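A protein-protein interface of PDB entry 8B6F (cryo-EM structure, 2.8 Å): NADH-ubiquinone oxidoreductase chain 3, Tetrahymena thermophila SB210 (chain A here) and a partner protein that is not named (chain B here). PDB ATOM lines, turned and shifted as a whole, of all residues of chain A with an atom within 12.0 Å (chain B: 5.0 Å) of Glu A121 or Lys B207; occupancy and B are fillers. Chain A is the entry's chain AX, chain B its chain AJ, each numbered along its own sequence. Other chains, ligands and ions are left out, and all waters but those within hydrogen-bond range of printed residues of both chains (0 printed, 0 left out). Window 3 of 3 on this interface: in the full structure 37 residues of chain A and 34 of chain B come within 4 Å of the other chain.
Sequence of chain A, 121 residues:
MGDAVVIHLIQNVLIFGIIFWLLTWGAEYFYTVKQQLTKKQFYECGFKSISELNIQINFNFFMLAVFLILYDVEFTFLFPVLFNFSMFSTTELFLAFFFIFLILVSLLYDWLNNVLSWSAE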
ATOM      1  N   GLN A  56      39.087 -18.941 -11.759  1.00  0.00           N
ATOM      2  CA  GLN A  56      37.878 -18.855 -12.568  1.00  0.00           C
ATOM      3  C   GLN A  56      38.190 -18.344 -13.968  1.00  0.00           C
ATOM      4  O   GLN A  56      38.960 -17.397 -14.147  1.00  0.00           O
ATOM      5  CB  GLN A  56      36.862 -17.928 -11.894  1.00  0.00           C
ATOM      6  CG  GLN A  56      35.597 -17.706 -12.708  1.00  0.00           C
ATOM      7  CD  GLN A  56      34.595 -16.828 -11.995  1.00  0.00           C
ATOM      8  OE1 GLN A  56      34.832 -16.376 -10.878  1.00  0.00           O
ATOM      9  NE2 GLN A  56      33.460 -16.585 -12.639  1.00  0.00           N
ATOM     10  N   ILE A  57      37.584 -18.986 -14.962  1.00  0.00           N
ATOM     11  CA  ILE A  57      37.685 -18.565 -16.350  1.00  0.00           C
ATOM     12  C   ILE A  57      36.373 -17.906 -16.761  1.00  0.00           C
ATOM     13  O   ILE A  57      35.361 -17.992 -16.067  1.00  0.00           O
ATOM     14  CB  ILE A  57      38.019 -19.733 -17.294  1.00  0.00           C
ATOM     15  CG1 ILE A  57      37.024 -20.880 -17.096  1.00  0.00           C
ATOM     16  CG2 ILE A  57      39.453 -20.173 -17.098  1.00  0.00           C
ATOM     17  CD1 ILE A  57      36.337 -21.294 -18.366  1.00  0.00           C
ATOM     18  N   ASN A  58      36.402 -17.241 -17.911  1.00  0.00           N
ATOM     19  CA  ASN A  58      35.226 -16.590 -18.469  1.00  0.00           C
ATOM     20  C   ASN A  58      34.647 -17.484 -19.558  1.00  0.00           C
ATOM     21  O   ASN A  58      35.321 -17.775 -20.552  1.00  0.00           O
ATOM     22  CB  ASN A  58      35.579 -15.214 -19.029  1.00  0.00           C
ATOM     23  CG  ASN A  58      34.354 -14.406 -19.397  1.00  0.00           C
ATOM     24  OD1 ASN A  58      33.234 -14.751 -19.027  1.00  0.00           O
ATOM     25  ND2 ASN A  58      34.562 -13.318 -20.128  1.00  0.00           N
ATOM     26  N   PHE A  59      33.409 -17.924 -19.361  1.00  0.00           N
ATOM     27  CA  PHE A  59      32.736 -18.815 -20.300  1.00  0.00           C
ATOM     28  C   PHE A  59      31.836 -17.987 -21.216  1.00  0.00           C
ATOM     29  O   PHE A  59      30.609 -18.066 -21.182  1.00  0.00           O
ATOM     30  CB  PHE A  59      31.949 -19.876 -19.533  1.00  0.00           C
ATOM     31  CG  PHE A  59      31.450 -21.020 -20.377  1.00  0.00           C
ATOM     32  CD1 PHE A  59      31.882 -21.204 -21.681  1.00  0.00           C
ATOM     33  CD2 PHE A  59      30.536 -21.915 -19.848  1.00  0.00           C
ATOM     34  CE1 PHE A  59      31.411 -22.261 -22.435  1.00  0.00           C
ATOM     35  CE2 PHE A  59      30.064 -22.973 -20.596  1.00  0.00           C
ATOM     36  CZ  PHE A  59      30.501 -23.147 -21.891  1.00  0.00           C
ATOM     37  N   ASN A  60      32.483 -17.173 -22.045  1.00  0.00           N
ATOM     38  CA  ASN A  60      31.787 -16.260 -22.943  1.00  0.00           C
ATOM     39  C   ASN A  60      31.460 -16.892 -24.289  1.00  0.00           C
ATOM     40  O   ASN A  60      30.965 -16.195 -25.181  1.00  0.00           O
ATOM     41  CB  ASN A  60      32.612 -14.986 -23.147  1.00  0.00           C
ATOM     42  CG  ASN A  60      34.022 -15.270 -23.608  1.00  0.00           C
ATOM     43  OD1 ASN A  60      34.327 -16.369 -24.066  1.00  0.00           O
ATOM     44  ND2 ASN A  60      34.894 -14.277 -23.487  1.00  0.00           N
ATOM     45  N   PHE A  61      31.726 -18.186 -24.458  1.00  0.00           N
ATOM     46  CA  PHE A  61      31.364 -18.918 -25.665  1.00  0.00           C
ATOM     47  C   PHE A  61      30.359 -20.023 -25.353  1.00  0.00           C
ATOM     48  O   PHE A  61      30.321 -21.050 -26.031  1.00  0.00           O
ATOM     49  CB  PHE A  61      32.607 -19.497 -26.339  1.00  0.00           C
ATOM     50  CG  PHE A  61      33.382 -20.447 -25.472  1.00  0.00           C
ATOM     51  CD1 PHE A  61      34.360 -19.976 -24.614  1.00  0.00           C
ATOM     52  CD2 PHE A  61      33.141 -21.809 -25.523  1.00  0.00           C
ATOM     53  CE1 PHE A  61      35.078 -20.844 -23.816  1.00  0.00           C
ATOM     54  CE2 PHE A  61      33.856 -22.683 -24.728  1.00  0.00           C
ATOM     55  CZ  PHE A  61      34.826 -22.199 -23.874  1.00  0.00           C
ATOM     56  N   PHE A  62      29.531 -19.817 -24.326  1.00  0.00           N
ATOM     57  CA  PHE A  62      28.607 -20.853 -23.884  1.00  0.00           C
ATOM     58  C   PHE A  62      27.498 -21.126 -24.889  1.00  0.00           C
ATOM     59  O   PHE A  62      26.897 -22.204 -24.845  1.00  0.00           O
ATOM     60  CB  PHE A  62      27.992 -20.473 -22.536  1.00  0.00           C
ATOM     61  CG  PHE A  62      27.159 -19.224 -22.575  1.00  0.00           C
ATOM     62  CD1 PHE A  62      25.800 -19.292 -22.837  1.00  0.00           C
ATOM     63  CD2 PHE A  62      27.724 -17.987 -22.320  1.00  0.00           C
ATOM     64  CE1 PHE A  62      25.027 -18.151 -22.864  1.00  0.00           C
ATOM     65  CE2 PHE A  62      26.956 -16.840 -22.344  1.00  0.00           C
ATOM     66  CZ  PHE A  62      25.606 -16.922 -22.616  1.00  0.00           C
ATOM     67  N   MET A  63      27.210 -20.188 -25.792  1.00  0.00           N
ATOM     68  CA  MET A  63      26.185 -20.439 -26.799  1.00  0.00           C
ATOM     69  C   MET A  63      26.572 -21.594 -27.707  1.00  0.00           C
ATOM     70  O   MET A  63      25.702 -22.334 -28.178  1.00  0.00           O
ATOM     71  CB  MET A  63      25.939 -19.180 -27.627  1.00  0.00           C
ATOM     72  CG  MET A  63      25.350 -18.023 -26.840  1.00  0.00           C
ATOM     73  SD  MET A  63      23.809 -18.439 -25.998  1.00  0.00           S
ATOM     74  CE  MET A  63      22.806 -19.022 -27.360  1.00  0.00           C
ATOM     75  N   LEU A  64      27.867 -21.765 -27.965  1.00  0.00           N
ATOM     76  CA  LEU A  64      28.311 -22.878 -28.792  1.00  0.00           C
ATOM     77  C   LEU A  64      27.984 -24.213 -28.139  1.00  0.00           C
ATOM     78  O   LEU A  64      27.517 -25.142 -28.807  1.00  0.00           O
ATOM     79  CB  LEU A  64      29.806 -22.751 -29.050  1.00  0.00           C
ATOM     80  CG  LEU A  64      30.185 -21.489 -29.822  1.00  0.00           C
ATOM     81  CD1 LEU A  64      31.669 -21.351 -29.777  1.00  0.00           C
ATOM     82  CD2 LEU A  64      29.691 -21.536 -31.259  1.00  0.00           C
ATOM     83  N   ASN A 113      21.690 -13.866 -35.907  1.00  0.00           N
ATOM     84  CA  ASN A 113      21.758 -13.200 -34.614  1.00  0.00           C
ATOM     85  C   ASN A 113      23.178 -13.078 -34.076  1.00  0.00           C
ATOM     86  O   ASN A 113      23.383 -12.381 -33.077  1.00  0.00           O
ATOM     87  CB  ASN A 113      20.885 -13.942 -33.605  1.00  0.00           C
ATOM     88  CG  ASN A 113      19.429 -13.559 -33.719  1.00  0.00           C
ATOM     89  OD1 ASN A 113      18.930 -12.738 -32.953  1.00  0.00           O
ATOM     90  ND2 ASN A 113      18.740 -14.146 -34.689  1.00  0.00           N
ATOM     91  N   ASN A 114      24.156 -13.727 -34.705  1.00  0.00           N
ATOM     92  CA  ASN A 114      25.566 -13.553 -34.355  1.00  0.00           C
ATOM     93  C   ASN A 114      25.842 -14.027 -32.930  1.00  0.00           C
ATOM     94  O   ASN A 114      26.488 -13.343 -32.135  1.00  0.00           O
ATOM     95  CB  ASN A 114      26.003 -12.098 -34.537  1.00  0.00           C
ATOM     96  CG  ASN A 114      25.781 -11.597 -35.949  1.00  0.00           C
ATOM     97  OD1 ASN A 114      25.170 -10.551 -36.160  1.00  0.00           O
ATOM     98  ND2 ASN A 114      26.274 -12.349 -36.928  1.00  0.00           N
ATOM     99  N   VAL A 115      25.339 -15.220 -32.612  1.00  0.00           N
ATOM    100  CA  VAL A 115      25.577 -15.839 -31.314  1.00  0.00           C
ATOM    101  C   VAL A 115      26.655 -16.907 -31.378  1.00  0.00           C
ATOM    102  O   VAL A 115      26.910 -17.582 -30.373  1.00  0.00           O
ATOM    103  CB  VAL A 115      24.277 -16.436 -30.735  1.00  0.00           C
ATOM    104  CG1 VAL A 115      23.324 -15.327 -30.326  1.00  0.00           C
ATOM    105  CG2 VAL A 115      23.610 -17.361 -31.743  1.00  0.00           C
ATOM    106  N   LEU A 116      27.305 -17.075 -32.531  1.00  0.00           N
ATOM    107  CA  LEU A 116      28.339 -18.083 -32.728  1.00  0.00           C
ATOM    108  C   LEU A 116      29.742 -17.497 -32.619  1.00  0.00           C
ATOM    109  O   LEU A 116      30.680 -18.018 -33.229  1.00  0.00           O
ATOM    110  CB  LEU A 116      28.155 -18.763 -34.084  1.00  0.00           C
ATOM    111  CG  LEU A 116      26.781 -19.381 -34.357  1.00  0.00           C
ATOM    112  CD1 LEU A 116      26.704 -19.902 -35.780  1.00  0.00           C
ATOM    113  CD2 LEU A 116      26.481 -20.494 -33.366  1.00  0.00           C
ATOM    114  N   SER A 117      29.904 -16.416 -31.859  1.00  0.00           N
ATOM    115  CA  SER A 117      31.190 -15.750 -31.726  1.00  0.00           C
ATOM    116  C   SER A 117      31.374 -15.290 -30.287  1.00  0.00           C
ATOM    117  O   SER A 117      30.414 -15.164 -29.525  1.00  0.00           O
ATOM    118  CB  SER A 117      31.309 -14.557 -32.682  1.00  0.00           C
ATOM    119  OG  SER A 117      30.281 -13.610 -32.444  1.00  0.00           O
ATOM    120  N   TRP A 118      32.631 -15.039 -29.927  1.00  0.00           N
ATOM    121  CA  TRP A 118      32.947 -14.577 -28.583  1.00  0.00           C
ATOM    122  C   TRP A 118      32.338 -13.203 -28.332  1.00  0.00           C
ATOM    123  O   TRP A 118      32.276 -12.357 -29.229  1.00  0.00           O
ATOM    124  CB  TRP A 118      34.464 -14.525 -28.392  1.00  0.00           C
ATOM    125  CG  TRP A 118      35.051 -15.815 -27.912  1.00  0.00           C
ATOM    126  CD1 TRP A 118      35.715 -16.022 -26.740  1.00  0.00           C
ATOM    127  CD2 TRP A 118      35.025 -17.078 -28.588  1.00  0.00           C
ATOM    128  NE1 TRP A 118      36.106 -17.336 -26.645  1.00  0.00           N
ATOM    129  CE2 TRP A 118      35.694 -18.005 -27.766  1.00  0.00           C
ATOM    130  CE3 TRP A 118      34.501 -17.515 -29.809  1.00  0.00           C
ATOM    131  CZ2 TRP A 118      35.853 -19.342 -28.124  1.00  0.00           C
ATOM    132  CZ3 TRP A 118      34.659 -18.843 -30.163  1.00  0.00           C
ATOM    133  CH2 TRP A 118      35.330 -19.742 -29.323  1.00  0.00           C
ATOM    134  N   SER A 119      31.884 -12.986 -27.102  1.00  0.00           N
ATOM    135  CA  SER A 119      31.243 -11.746 -26.695  1.00  0.00           C
ATOM    136  C   SER A 119      32.027 -11.112 -25.554  1.00  0.00           C
ATOM    137  O   SER A 119      32.932 -11.717 -24.977  1.00  0.00           O
ATOM    138  CB  SER A 119      29.789 -11.990 -26.275  1.00  0.00           C
ATOM    139  OG  SER A 119      29.713 -12.926 -25.214  1.00  0.00           O
ATOM    140  N   ALA A 120      31.662  -9.869 -25.231  1.00  0.00           N
ATOM    141  CA  ALA A 120      32.384  -9.131 -24.199  1.00  0.00           C
ATOM    142  C   ALA A 120      32.313  -9.844 -22.855  1.00  0.00           C
ATOM    143  O   ALA A 120      33.316  -9.929 -22.136  1.00  0.00           O
ATOM    144  CB  ALA A 120      31.823  -7.715 -24.080  1.00  0.00           C
ATOM    145  N   GLU A 121      31.141 -10.357 -22.495  1.00  0.00           N
ATOM    146  CA  GLU A 121      30.979 -11.084 -21.242  1.00  0.00           C
ATOM    147  C   GLU A 121      30.097 -12.309 -21.444  1.00  0.00           C
ATOM    148  O   GLU A 121      30.286 -13.337 -20.793  1.00  0.00           O
ATOM    149  CB  GLU A 121      30.380 -10.173 -20.167  1.00  0.00           C
ATOM    150  CG  GLU A 121      30.343 -10.796 -18.776  1.00  0.00           C
ATOM    151  CD  GLU A 121      31.726 -10.999 -18.188  1.00  0.00           C
ATOM    152  OE1 GLU A 121      32.712 -10.557 -18.813  1.00  0.00           O
ATOM    153  OE2 GLU A 121      31.827 -11.600 -17.098  1.00  0.00           O
ATOM    154  OXT GLU A 121      29.179 -12.304 -22.264  1.00  0.00           O
ATOM    155  N   TYR B 102      33.374 -22.528 -15.019  1.00  0.00           N
ATOM    156  CA  TYR B 102      32.947 -21.136 -15.096  1.00  0.00           C
ATOM    157  C   TYR B 102      32.397 -20.653 -13.761  1.00  0.00           C
ATOM    158  O   TYR B 102      32.806 -19.604 -13.251  1.00  0.00           O
ATOM    159  CB  TYR B 102      31.898 -20.976 -16.194  1.00  0.00           C
ATOM    160  CG  TYR B 102      31.358 -19.571 -16.318  1.00  0.00           C
ATOM    161  CD1 TYR B 102      32.202 -18.472 -16.224  1.00  0.00           C
ATOM    162  CD2 TYR B 102      30.007 -19.342 -16.540  1.00  0.00           C
ATOM    163  CE1 TYR B 102      31.716 -17.186 -16.341  1.00  0.00           C
ATOM    164  CE2 TYR B 102      29.511 -18.060 -16.658  1.00  0.00           C
ATOM    165  CZ  TYR B 102      30.371 -16.986 -16.558  1.00  0.00           C
ATOM    166  OH  TYR B 102      29.882 -15.709 -16.676  1.00  0.00           O
ATOM    167  N   TYR B 203      19.772 -15.180 -24.506  1.00  0.00           N
ATOM    168  CA  TYR B 203      21.112 -14.606 -24.535  1.00  0.00           C
ATOM    169  C   TYR B 203      21.058 -13.093 -24.717  1.00  0.00           C
ATOM    170  O   TYR B 203      21.779 -12.353 -24.038  1.00  0.00           O
ATOM    171  CB  TYR B 203      21.923 -15.254 -25.655  1.00  0.00           C
ATOM    172  CG  TYR B 203      23.267 -14.612 -25.901  1.00  0.00           C
ATOM    173  CD1 TYR B 203      24.380 -14.975 -25.156  1.00  0.00           C
ATOM    174  CD2 TYR B 203      23.425 -13.651 -26.890  1.00  0.00           C
ATOM    175  CE1 TYR B 203      25.609 -14.394 -25.382  1.00  0.00           C
ATOM    176  CE2 TYR B 203      24.648 -13.064 -27.125  1.00  0.00           C
ATOM    177  CZ  TYR B 203      25.736 -13.439 -26.368  1.00  0.00           C
ATOM    178  OH  TYR B 203      26.958 -12.855 -26.600  1.00  0.00           O
ATOM    179  N   LYS B 204      20.213 -12.614 -25.632  1.00  0.00           N
ATOM    180  CA  LYS B 204      20.080 -11.176 -25.831  1.00  0.00           C
ATOM    181  C   LYS B 204      19.545 -10.497 -24.577  1.00  0.00           C
ATOM    182  O   LYS B 204      19.993  -9.406 -24.213  1.00  0.00           O
ATOM    183  CB  LYS B 204      19.175 -10.887 -27.027  1.00  0.00           C
ATOM    184  CG  LYS B 204      19.766 -11.325 -28.360  1.00  0.00           C
ATOM    185  CD  LYS B 204      18.920 -10.862 -29.537  1.00  0.00           C
ATOM    186  CE  LYS B 204      17.556 -11.535 -29.553  1.00  0.00           C
ATOM    187  NZ  LYS B 204      16.752 -11.139 -30.745  1.00  0.00           N
ATOM    188  N   SER B 205      18.572 -11.123 -23.911  1.00  0.00           N
ATOM    189  CA  SER B 205      18.036 -10.555 -22.679  1.00  0.00           C
ATOM    190  C   SER B 205      19.109 -10.468 -21.604  1.00  0.00           C
ATOM    191  O   SER B 205      19.182  -9.480 -20.865  1.00  0.00           O
ATOM    192  CB  SER B 205      16.853 -11.387 -22.185  1.00  0.00           C
ATOM    193  OG  SER B 205      15.817 -11.419 -23.151  1.00  0.00           O
ATOM    194  N   ASN B 206      19.947 -11.499 -21.494  1.00  0.00           N
ATOM    195  CA  ASN B 206      21.062 -11.445 -20.558  1.00  0.00           C
ATOM    196  C   ASN B 206      22.012 -10.307 -20.906  1.00  0.00           C
ATOM    197  O   ASN B 206      22.511  -9.609 -20.015  1.00  0.00           O
ATOM    198  CB  ASN B 206      21.799 -12.785 -20.558  1.00  0.00           C
ATOM    199  CG  ASN B 206      22.965 -12.808 -19.594  1.00  0.00           C
ATOM    200  OD1 ASN B 206      22.804 -13.122 -18.416  1.00  0.00           O
ATOM    201  ND2 ASN B 206      24.151 -12.486 -20.093  1.00  0.00           N
ATOM    202  N   LYS B 207      22.276 -10.104 -22.198  1.00  0.00           N
ATOM    203  CA  LYS B 207      23.164  -9.025 -22.616  1.00  0.00           C
ATOM    204  C   LYS B 207      22.590  -7.659 -22.260  1.00  0.00           C
ATOM    205  O   LYS B 207      23.335  -6.738 -21.916  1.00  0.00           O
ATOM    206  CB  LYS B 207      23.429  -9.115 -24.119  1.00  0.00           C
ATOM    207  CG  LYS B 207      24.671  -9.910 -24.482  1.00  0.00           C
ATOM    208  CD  LYS B 207      25.939  -9.142 -24.139  1.00  0.00           C
ATOM    209  CE  LYS B 207      27.183  -9.929 -24.513  1.00  0.00           C
ATOM    210  NZ  LYS B 207      27.300 -11.198 -23.742  1.00  0.00           N
ATOM    211  N   ASN B 208      21.270  -7.500 -22.353  1.00  0.00           N
ATOM    212  CA  ASN B 208      20.673  -6.183 -22.162  1.00  0.00           C
ATOM    213  C   ASN B 208      21.018  -5.571 -20.809  1.00  0.00           C
ATOM    214  O   ASN B 208      21.016  -4.343 -20.685  1.00  0.00           O
ATOM    215  CB  ASN B 208      19.152  -6.259 -22.313  1.00  0.00           C
ATOM    216  CG  ASN B 208      18.717  -6.458 -23.753  1.00  0.00           C
ATOM    217  OD1 ASN B 208      19.372  -5.990 -24.684  1.00  0.00           O
ATOM    218  ND2 ASN B 208      17.599  -7.150 -23.942  1.00  0.00           N
ATOM    219  N   TYR B 209      21.338  -6.388 -19.804  1.00  0.00           N
ATOM    220  CA  TYR B 209      21.619  -5.851 -18.475  1.00  0.00           C
ATOM    221  C   TYR B 209      22.808  -4.898 -18.495  1.00  0.00           C
ATOM    222  O   TYR B 209      22.772  -3.838 -17.863  1.00  0.00           O
ATOM    223  CB  TYR B 209      21.863  -6.991 -17.487  1.00  0.00           C
ATOM    224  CG  TYR B 209      20.590  -7.604 -16.958  1.00  0.00           C
ATOM    225  CD1 TYR B 209      19.959  -7.080 -15.837  1.00  0.00           C
ATOM    226  CD2 TYR B 209      20.015  -8.704 -17.579  1.00  0.00           C
ATOM    227  CE1 TYR B 209      18.793  -7.634 -15.350  1.00  0.00           C
ATOM    228  CE2 TYR B 209      18.848  -9.265 -17.100  1.00  0.00           C
ATOM    229  CZ  TYR B 209      18.243  -8.725 -15.985  1.00  0.00           C
ATOM    230  OH  TYR B 209      17.083  -9.277 -15.501  1.00  0.00           O
ATOM    231  N   THR B 210      23.874  -5.260 -19.209  1.00  0.00           N
ATOM    232  CA  THR B 210      25.024  -4.370 -19.320  1.00  0.00           C
ATOM    233  C   THR B 210      24.760  -3.198 -20.256  1.00  0.00           C
ATOM    234  O   THR B 210      25.461  -2.187 -20.173  1.00  0.00           O
ATOM    235  CB  THR B 210      26.266  -5.140 -19.783  1.00  0.00           C
ATOM    236  OG1 THR B 210      27.350  -4.226 -19.991  1.00  0.00           O
ATOM    237  CG2 THR B 210      26.005  -5.905 -21.067  1.00  0.00           C
ATOM    238  N   ILE B 211      23.763  -3.307 -21.137  1.00  0.00           N
ATOM    239  CA  ILE B 211      23.438  -2.215 -22.048  1.00  0.00           C
ATOM    240  C   ILE B 211      22.582  -1.142 -21.386  1.00  0.00           C
ATOM    241  O   ILE B 211      22.530  -0.012 -21.884  1.00  0.00           O
ATOM    242  CB  ILE B 211      22.708  -2.754 -23.293  1.00  0.00           C
ATOM    243  CG1 ILE B 211      23.558  -3.815 -23.997  1.00  0.00           C
ATOM    244  CG2 ILE B 211      22.370  -1.621 -24.258  1.00  0.00           C
ATOM    245  CD1 ILE B 211      22.836  -4.539 -25.121  1.00  0.00           C
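Printed residues of chain A that touch a printed residue of chain B: Gln A56, Ile A57, Asn A58, Phe A59, Phe A62, Met A63, Asn A113, Val A115, Ser A119 and Glu A121. Hydrophobic or aromatic side chains of chain A within 4 Å of the printed part of chain B: Phe A59, Phe A62, Met A63 and Val A115. Of the 10 printed residues of chain B, 4 touch a printed residue of chain A. Hydrophobic or aromatic side chains of chain B that line the printed part of chain A: Tyr B102 and Tyr B203. Along chain B the printed residues that touch a printed residue of chain A span positions 102 to 207. Among the printed residues, 11 pairs touch across the chains. Among the printed residues, no Asp or Glu carboxylate lies within 4 Å of a Lys or Arg side-chain nitrogen of the other chain.
The side-chain hydroxyl (OH) of Tyr B203 sits close to the side-chain hydroxyl (OG) of Ser A119 (3.1 Å). The side-chain amino group (NZ) of Lys B204 lies within hydrogen-bond range of the side-chain amide oxygen (OD1) of Asn A113, at 3.5 Å. The backbone carbonyl oxygen (O) of Tyr B102 sits at hydrogen-bond distance from the side-chain amide nitrogen (NE2) of Gln A56, 3.1 Å away. NZ of Lys B207 sits at hydrogen-bond distance from OG of Ser A119, 3.3 Å away. The side-chain amino group of Lys B207 is in salt-bridge range of the chain-end carboxylate of Glu A121 (2.6 Å).
The side-chain hydroxyl (OH) of Tyr B203 sits at hydrogen-bond distance from the side-chain amino group (NZ) of Lys B207, 3.3 Å away. The backbone carbonyl oxygen (O) of Lys B204 lies close to the side-chain amide nitrogen (ND2) of Asn B208 (3.3 Å). OG of Ser A119 sits at hydrogen-bond distance from OXT of Glu A121, at 3.1 Å.
O of Ile A57 touches CD1 of Tyr B102, at 3.2 Å. OD1 of Asn A58 touches CE1 of Tyr B102 (3.9 Å). CB of Phe A59 touches CG of Tyr B102 (3.3 Å). CZ of Phe A62 touches CD1 of Tyr B203, 3.4 Å away. Tyr B203 touches Met A63. Val A115 touches Tyr B203.
Printed residues of chain B within 4 Å of Ile A57: Tyr B102. Printed residues of chain B within 4 Å of Met A63: Tyr B203. Of the printed residues of chain B, Asn A113 touches Lys B204. Leu A116 touches none of the printed residues of chain B. Ala A120 touches none of the printed residues of chain B. Glu A121 touches just one residue of chain B: Lys B207 (2.6 Å). Tyr B203 touches just these residues of chain A: Phe A62 (3.4 Å), Met A63 (3.6 Å), Val A115 (3.8 Å) and Ser A119 (3.0 Å). Of the printed residues of chain A, Lys B204 touches Asn A113. Ser B205 touches none of the printed residues of chain A. No residue of chain A comes within 4 Å of Asn B206. Of chain A, only Ser A119 and Glu A121 come within 4 Å of Lys B207. No residue of chain A comes within 4 Å of Asn B208. No residue of chain A comes within 4 Å of Thr B210. No residue of chain A comes within 4 Å of Ile B211. The nearest residue of chain B that does not touch Glu A121 is Tyr B102 (4.6 Å). The nearest residue of chain A that does not touch Lys B207 is Ala A120 (4.5 Å).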
